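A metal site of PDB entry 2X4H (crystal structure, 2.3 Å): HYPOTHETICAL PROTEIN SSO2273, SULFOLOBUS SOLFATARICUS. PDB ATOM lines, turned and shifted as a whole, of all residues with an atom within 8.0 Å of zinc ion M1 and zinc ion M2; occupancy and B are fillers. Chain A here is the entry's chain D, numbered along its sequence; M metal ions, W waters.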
ATOM      1  N   ARG A  13      13.872  34.085  29.244  1.00  0.00           N
ATOM      2  CA  ARG A  13      15.273  34.470  29.409  1.00  0.00           C
ATOM      3  C   ARG A  13      15.460  35.494  30.529  1.00  0.00           C
ATOM      4  O   ARG A  13      16.512  35.542  31.160  1.00  0.00           O
ATOM      5  CB  ARG A  13      15.913  34.975  28.107  1.00  0.00           C
ATOM      6  CG  ARG A  13      16.814  33.921  27.468  1.00  0.00           C
ATOM      7  CD  ARG A  13      17.792  34.457  26.442  1.00  0.00           C
ATOM      8  NE  ARG A  13      18.713  33.388  26.017  1.00  0.00           N
ATOM      9  CZ  ARG A  13      19.805  33.005  26.677  1.00  0.00           C
ATOM     10  NH1 ARG A  13      20.174  33.608  27.811  1.00  0.00           N
ATOM     11  NH2 ARG A  13      20.545  32.019  26.215  1.00  0.00           N
ATOM     12  N   ILE A  82      20.502  26.220  28.965  1.00  0.00           N
ATOM     13  CA  ILE A  82      21.916  26.088  28.571  1.00  0.00           C
ATOM     14  C   ILE A  82      22.083  25.080  27.432  1.00  0.00           C
ATOM     15  O   ILE A  82      22.678  25.397  26.389  1.00  0.00           O
ATOM     16  CB  ILE A  82      22.827  25.743  29.814  1.00  0.00           C
ATOM     17  CG1 ILE A  82      22.954  26.975  30.703  1.00  0.00           C
ATOM     18  CG2 ILE A  82      24.204  25.270  29.376  1.00  0.00           C
ATOM     19  CD1 ILE A  82      23.665  26.745  32.046  1.00  0.00           C
ATOM     20  N   HIS A  85      20.555  26.514  24.198  1.00  0.00           N
ATOM     21  CA  HIS A  85      21.440  27.563  23.679  1.00  0.00           C
ATOM     22  C   HIS A  85      22.599  26.951  22.939  1.00  0.00           C
ATOM     23  O   HIS A  85      22.864  27.308  21.794  1.00  0.00           O
ATOM     24  CB  HIS A  85      21.989  28.429  24.833  1.00  0.00           C
ATOM     25  CG  HIS A  85      23.084  29.383  24.444  1.00  0.00           C
ATOM     26  ND1 HIS A  85      22.875  30.476  23.627  1.00  0.00           N
ATOM     27  CD2 HIS A  85      24.386  29.434  24.815  1.00  0.00           C
ATOM     28  CE1 HIS A  85      24.010  31.142  23.499  1.00  0.00           C
ATOM     29  NE2 HIS A  85      24.948  30.530  24.209  1.00  0.00           N
ATOM     30  N   ARG A  86      23.281  25.999  23.589  1.00  0.00           N
ATOM     31  CA  ARG A  86      24.500  25.397  22.992  1.00  0.00           C
ATOM     32  C   ARG A  86      24.226  24.416  21.865  1.00  0.00           C
ATOM     33  O   ARG A  86      25.007  24.322  20.916  1.00  0.00           O
ATOM     34  CB  ARG A  86      25.375  24.764  24.083  1.00  0.00           C
ATOM     35  CG  ARG A  86      25.908  25.821  25.072  1.00  0.00           C
ATOM     36  CD  ARG A  86      26.617  25.220  26.289  1.00  0.00           C
ATOM     37  NE  ARG A  86      26.940  26.285  27.231  1.00  0.00           N
ATOM     38  CZ  ARG A  86      27.302  26.146  28.498  1.00  0.00           C
ATOM     39  NH1 ARG A  86      27.431  24.935  29.045  1.00  0.00           N
ATOM     40  NH2 ARG A  86      27.531  27.226  29.221  1.00  0.00           N
ATOM     41  N   VAL A  87      23.100  23.703  21.927  1.00  0.00           N
ATOM     42  CA  VAL A  87      22.746  22.851  20.788  1.00  0.00           C
ATOM     43  C   VAL A  87      22.445  23.728  19.558  1.00  0.00           C
ATOM     44  O   VAL A  87      22.819  23.390  18.460  1.00  0.00           O
ATOM     45  CB  VAL A  87      21.543  21.926  21.088  1.00  0.00           C
ATOM     46  CG1 VAL A  87      21.040  21.281  19.801  1.00  0.00           C
ATOM     47  CG2 VAL A  87      21.938  20.869  22.084  1.00  0.00           C
ATOM     48  N   GLU A  89      23.667  26.690  18.892  1.00  0.00           N
ATOM     49  CA  GLU A  89      24.922  27.283  18.425  1.00  0.00           C
ATOM     50  C   GLU A  89      25.679  26.390  17.496  1.00  0.00           C
ATOM     51  O   GLU A  89      26.307  26.885  16.542  1.00  0.00           O
ATOM     52  CB  GLU A  89      25.864  27.564  19.578  1.00  0.00           C
ATOM     53  CG  GLU A  89      25.461  28.695  20.415  1.00  0.00           C
ATOM     54  CD  GLU A  89      26.544  29.106  21.376  1.00  0.00           C
ATOM     55  OE1 GLU A  89      27.150  28.262  22.014  1.00  0.00           O
ATOM     56  OE2 GLU A  89      26.794  30.297  21.476  1.00  0.00           O
ATOM     57  N   ILE A  90      25.674  25.096  17.783  1.00  0.00           N
ATOM     58  CA  ILE A  90      26.376  24.127  16.922  1.00  0.00           C
ATOM     59  C   ILE A  90      25.723  24.116  15.541  1.00  0.00           C
ATOM     60  O   ILE A  90      26.426  24.154  14.504  1.00  0.00           O
ATOM     61  CB  ILE A  90      26.389  22.737  17.517  1.00  0.00           C
ATOM     62  CG1 ILE A  90      27.224  22.726  18.809  1.00  0.00           C
ATOM     63  CG2 ILE A  90      26.988  21.694  16.519  1.00  0.00           C
ATOM     64  CD1 ILE A  90      27.325  21.375  19.481  1.00  0.00           C
ATOM     65  N   VAL A  93      26.758  27.357  13.781  1.00  0.00           N
ATOM     66  CA  VAL A  93      28.117  27.289  13.288  1.00  0.00           C
ATOM     67  C   VAL A  93      28.198  26.287  12.148  1.00  0.00           C
ATOM     68  O   VAL A  93      28.971  26.481  11.222  1.00  0.00           O
ATOM     69  CB  VAL A  93      29.148  26.996  14.392  1.00  0.00           C
ATOM     70  CG1 VAL A  93      30.553  26.770  13.801  1.00  0.00           C
ATOM     71  CG2 VAL A  93      29.168  28.171  15.417  1.00  0.00           C
ATOM     72  N   LYS A  99      30.824  31.990  15.215  1.00  0.00           N
ATOM     73  CA  LYS A  99      30.401  31.492  16.538  1.00  0.00           C
ATOM     74  C   LYS A  99      30.072  32.569  17.587  1.00  0.00           C
ATOM     75  O   LYS A  99      29.284  32.319  18.521  1.00  0.00           O
ATOM     76  CB  LYS A  99      31.463  30.552  17.099  1.00  0.00           C
ATOM     77  CG  LYS A  99      32.861  31.143  17.293  1.00  0.00           C
ATOM     78  CD  LYS A  99      33.877  30.010  17.283  1.00  0.00           C
ATOM     79  CE  LYS A  99      35.049  30.288  18.176  1.00  0.00           C
ATOM     80  NZ  LYS A  99      35.767  29.006  18.451  1.00  0.00           N
ATOM     81  N   GLN A 100      30.668  33.752  17.449  1.00  0.00           N
ATOM     82  CA  GLN A 100      30.329  34.871  18.308  1.00  0.00           C
ATOM     83  C   GLN A 100      28.937  35.381  17.915  1.00  0.00           C
ATOM     84  O   GLN A 100      28.125  35.767  18.769  1.00  0.00           O
ATOM     85  CB  GLN A 100      31.358  36.002  18.204  1.00  0.00           C
ATOM     86  CG  GLN A 100      32.840  35.566  18.195  1.00  0.00           C
ATOM     87  CD  GLN A 100      33.354  35.051  19.553  1.00  0.00           C
ATOM     88  OE1 GLN A 100      32.801  34.102  20.127  1.00  0.00           O
ATOM     89  NE2 GLN A 100      34.408  35.695  20.061  1.00  0.00           N
ATOM     90  N   ALA A 102      26.749  33.509  16.339  1.00  0.00           N
ATOM     91  CA  ALA A 102      25.870  32.381  16.666  1.00  0.00           C
ATOM     92  C   ALA A 102      25.416  32.417  18.138  1.00  0.00           C
ATOM     93  O   ALA A 102      24.272  32.113  18.422  1.00  0.00           O
ATOM     94  CB  ALA A 102      26.554  31.074  16.346  1.00  0.00           C
ATOM     95  N   CYS A 103      26.303  32.794  19.053  1.00  0.00           N
ATOM     96  CA  CYS A 103      25.951  32.883  20.488  1.00  0.00           C
ATOM     97  C   CYS A 103      24.874  33.958  20.718  1.00  0.00           C
ATOM     98  O   CYS A 103      23.766  33.691  21.215  1.00  0.00           O
ATOM     99  CB  CYS A 103      27.189  33.243  21.282  1.00  0.00           C
ATOM    100  SG  CYS A 103      26.919  33.328  23.050  1.00  0.00           S
ATOM    101  N   GLU A 104      25.194  35.177  20.307  1.00  0.00           N
ATOM    102  CA  GLU A 104      24.238  36.273  20.362  1.00  0.00           C
ATOM    103  C   GLU A 104      22.922  35.956  19.593  1.00  0.00           C
ATOM    104  O   GLU A 104      21.823  36.162  20.109  1.00  0.00           O
ATOM    105  CB  GLU A 104      24.924  37.523  19.840  1.00  0.00           C
ATOM    106  CG  GLU A 104      24.211  38.784  20.042  1.00  0.00           C
ATOM    107  CD  GLU A 104      23.911  39.102  21.500  1.00  0.00           C
ATOM    108  OE1 GLU A 104      24.613  38.621  22.442  1.00  0.00           O
ATOM    109  OE2 GLU A 104      22.952  39.882  21.652  1.00  0.00           O
ATOM    110  N   TYR A 105      22.994  35.403  18.385  1.00  0.00           N
ATOM    111  CA  TYR A 105      21.738  35.086  17.656  1.00  0.00           C
ATOM    112  C   TYR A 105      20.914  34.051  18.430  1.00  0.00           C
ATOM    113  O   TYR A 105      19.714  34.215  18.625  1.00  0.00           O
ATOM    114  CB  TYR A 105      22.001  34.502  16.265  1.00  0.00           C
ATOM    115  CG  TYR A 105      22.346  35.470  15.141  1.00  0.00           C
ATOM    116  CD1 TYR A 105      22.072  36.835  15.205  1.00  0.00           C
ATOM    117  CD2 TYR A 105      22.895  34.959  13.973  1.00  0.00           C
ATOM    118  CE1 TYR A 105      22.393  37.670  14.121  1.00  0.00           C
ATOM    119  CE2 TYR A 105      23.211  35.770  12.912  1.00  0.00           C
ATOM    120  CZ  TYR A 105      22.979  37.105  12.969  1.00  0.00           C
ATOM    121  OH  TYR A 105      23.333  37.842  11.849  1.00  0.00           O
ATOM    122  N   SER A 106      21.570  32.991  18.877  1.00  0.00           N
ATOM    123  CA  SER A 106      20.896  31.950  19.626  1.00  0.00           C
ATOM    124  C   SER A 106      20.056  32.484  20.804  1.00  0.00           C
ATOM    125  O   SER A 106      18.952  31.995  21.044  1.00  0.00           O
ATOM    126  CB  SER A 106      21.931  30.919  20.092  1.00  0.00           C
ATOM    127  OG  SER A 106      21.345  29.839  20.818  1.00  0.00           O
ATOM    128  N   LYS A 107      20.545  33.512  21.507  1.00  0.00           N
ATOM    129  CA  LYS A 107      19.817  34.061  22.662  1.00  0.00           C
ATOM    130  C   LYS A 107      18.483  34.717  22.298  1.00  0.00           C
ATOM    131  O   LYS A 107      17.586  34.837  23.135  1.00  0.00           O
ATOM    132  CB  LYS A 107      20.699  35.051  23.462  1.00  0.00           C
ATOM    133  CG  LYS A 107      21.995  34.409  24.011  1.00  0.00           C
ATOM    134  CD  LYS A 107      22.802  35.346  24.915  1.00  0.00           C
ATOM    135  CE  LYS A 107      24.191  34.766  25.210  1.00  0.00           C
ATOM    136  NZ  LYS A 107      24.683  35.022  26.594  1.00  0.00           N
ATOM    137  N   ASP A 110      16.416  30.822  21.547  1.00  0.00           N
ATOM    138  CA  ASP A 110      16.692  29.486  22.048  1.00  0.00           C
ATOM    139  C   ASP A 110      15.676  29.005  23.080  1.00  0.00           C
ATOM    140  O   ASP A 110      15.358  27.826  23.145  1.00  0.00           O
ATOM    141  CB  ASP A 110      18.139  29.344  22.563  1.00  0.00           C
ATOM    142  CG  ASP A 110      18.535  30.388  23.600  1.00  0.00           C
ATOM    143  OD1 ASP A 110      17.698  31.171  24.098  1.00  0.00           O
ATOM    144  OD2 ASP A 110      19.749  30.433  23.897  1.00  0.00           O
ATOM    145  N   TYR A 130      30.187  19.532  23.602  1.00  0.00           N
ATOM    146  CA  TYR A 130      30.672  20.906  23.736  1.00  0.00           C
ATOM    147  C   TYR A 130      30.013  21.809  22.699  1.00  0.00           C
ATOM    148  O   TYR A 130      29.846  21.399  21.551  1.00  0.00           O
ATOM    149  CB  TYR A 130      32.177  20.981  23.508  1.00  0.00           C
ATOM    150  CG  TYR A 130      33.036  20.112  24.403  1.00  0.00           C
ATOM    151  CD1 TYR A 130      33.218  20.425  25.759  1.00  0.00           C
ATOM    152  CD2 TYR A 130      33.668  18.979  23.903  1.00  0.00           C
ATOM    153  CE1 TYR A 130      34.010  19.617  26.577  1.00  0.00           C
ATOM    154  CE2 TYR A 130      34.463  18.166  24.707  1.00  0.00           C
ATOM    155  CZ  TYR A 130      34.631  18.494  26.048  1.00  0.00           C
ATOM    156  OH  TYR A 130      35.410  17.699  26.851  1.00  0.00           O
ATOM    157  N   CYS A 131      29.640  23.038  23.115  1.00  0.00           N
ATOM    158  CA  CYS A 131      29.323  24.098  22.191  1.00  0.00           C
ATOM    159  C   CYS A 131      30.604  24.503  21.459  1.00  0.00           C
ATOM    160  O   CYS A 131      31.693  24.144  21.899  1.00  0.00           O
ATOM    161  CB  CYS A 131      28.720  25.322  22.909  1.00  0.00           C
ATOM    162  SG  CYS A 131      29.928  26.450  23.683  1.00  0.00           S
ATOM    163  N   PRO A 132      30.474  25.273  20.355  1.00  0.00           N
ATOM    164  CA  PRO A 132      31.657  25.756  19.632  1.00  0.00           C
ATOM    165  C   PRO A 132      32.690  26.518  20.483  1.00  0.00           C
ATOM    166  O   PRO A 132      33.841  26.595  20.071  1.00  0.00           O
ATOM    167  CB  PRO A 132      31.047  26.703  18.589  1.00  0.00           C
ATOM    168  CG  PRO A 132      29.665  26.258  18.418  1.00  0.00           C
ATOM    169  CD  PRO A 132      29.241  25.793  19.767  1.00  0.00           C
ATOM    170  N   HIS A 133      32.290  27.062  21.644  1.00  0.00           N
ATOM    171  CA  HIS A 133      33.248  27.718  22.539  1.00  0.00           C
ATOM    172  C   HIS A 133      33.891  26.800  23.571  1.00  0.00           C
ATOM    173  O   HIS A 133      34.548  27.316  24.467  1.00  0.00           O
ATOM    174  CB  HIS A 133      32.593  28.821  23.348  1.00  0.00           C
ATOM    175  CG  HIS A 133      31.632  29.653  22.576  1.00  0.00           C
ATOM    176  ND1 HIS A 133      30.334  29.252  22.352  1.00  0.00           N
ATOM    177  CD2 HIS A 133      31.769  30.861  21.986  1.00  0.00           C
ATOM    178  CE1 HIS A 133      29.727  30.187  21.623  1.00  0.00           C
ATOM    179  NE2 HIS A 133      30.570  31.167  21.407  1.00  0.00           N
ATOM    180  N   GLY A 134      33.667  25.486  23.501  1.00  0.00           N
ATOM    181  CA  GLY A 134      34.214  24.547  24.508  1.00  0.00           C
ATOM    182  C   GLY A 134      33.424  24.352  25.809  1.00  0.00           C
ATOM    183  O   GLY A 134      33.813  23.550  26.659  1.00  0.00           O
ATOM    184  N   LEU A 135      32.306  25.065  25.986  1.00  0.00           N
ATOM    185  CA  LEU A 135      31.498  24.851  27.192  1.00  0.00           C
ATOM    186  C   LEU A 135      30.708  23.551  27.047  1.00  0.00           C
ATOM    187  O   LEU A 135      30.192  23.232  25.967  1.00  0.00           O
ATOM    188  CB  LEU A 135      30.584  26.021  27.509  1.00  0.00           C
ATOM    189  CG  LEU A 135      31.258  27.387  27.384  1.00  0.00           C
ATOM    190  CD1 LEU A 135      30.352  28.544  27.927  1.00  0.00           C
ATOM    191  CD2 LEU A 135      32.596  27.385  28.060  1.00  0.00           C
ATOM    192  N   GLU A 136      30.649  22.782  28.132  1.00  0.00           N
ATOM    193  CA  GLU A 136      30.105  21.437  28.114  1.00  0.00           C
ATOM    194  C   GLU A 136      28.578  21.524  27.944  1.00  0.00           C
ATOM    195  O   GLU A 136      27.989  22.516  28.310  1.00  0.00           O
ATOM    196  CB  GLU A 136      30.537  20.701  29.388  1.00  0.00           C
ATOM    197  CG  GLU A 136      32.077  20.613  29.546  1.00  0.00           C
ATOM    198  CD  GLU A 136      32.561  19.797  30.735  1.00  0.00           C
ATOM    199  OE1 GLU A 136      31.922  19.846  31.808  1.00  0.00           O
ATOM    200  OE2 GLU A 136      33.594  19.110  30.610  1.00  0.00           O
ATOM    201  N   ILE A 137      27.953  20.508  27.333  1.00  0.00           N
ATOM    202  CA  ILE A 137      26.500  20.512  27.075  1.00  0.00           C
ATOM    203  C   ILE A 137      25.756  19.496  27.963  1.00  0.00           C
ATOM    204  O   ILE A 137      25.854  18.296  27.723  1.00  0.00           O
ATOM    205  CB  ILE A 137      26.189  20.168  25.593  1.00  0.00           C
ATOM    206  CG1 ILE A 137      26.734  21.257  24.677  1.00  0.00           C
ATOM    207  CG2 ILE A 137      24.693  20.033  25.374  1.00  0.00           C
ATOM    208  CD1 ILE A 137      26.356  21.090  23.215  1.00  0.00           C
HETATM  209 ZN    ZN M   1      26.706  31.047  23.659  1.00  0.00          ZN
HETATM  210 ZN    ZN M   2      28.871  28.458  23.227  1.00  0.00          ZN
HETATM  211  O   HOH W   1      28.118  30.181  24.152  1.00  0.00           O
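A ring nitrogen (NE2) of His 133 lies within hydrogen-bond range of the backbone carbonyl oxygen (O) of Lys 99, 3.4 Å away.
O of His 85 lies within hydrogen-bond range of OG of Ser 106.
The side-chain carboxylate (OD2) of Asp 110 is in hydrogen-bond range of a ring nitrogen (ND1) of His 85 (3.1 Å).
SG of Cys 131 sits close to N of Leu 135, at 3.6 Å.
The nearest printed residue that does not touch zinc ion M2 is Arg 86 (4.4 Å).
Zinc ion M1 is bound by water W1 (1.7 Å), a ring nitrogen (NE2) of His 85 (1.9 Å), the side-chain carboxylate (OE2) of Glu 89 (2.3 Å) and the side-chain sulfur (SG) of Cys 103 (2.4 Å).
Zinc ion M1 has four donor atoms within binding distance.
Zinc ion M2 is bound by a ring nitrogen (ND1) of His 133 (1.9 Å), water W1 (2.1 Å), the side-chain carboxylate (OE1) of Glu 89 (2.1 Å) and the side-chain sulfur (SG) of Cys 131 (2.3 Å).
Zinc ion M2 has four donor atoms within binding distance.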
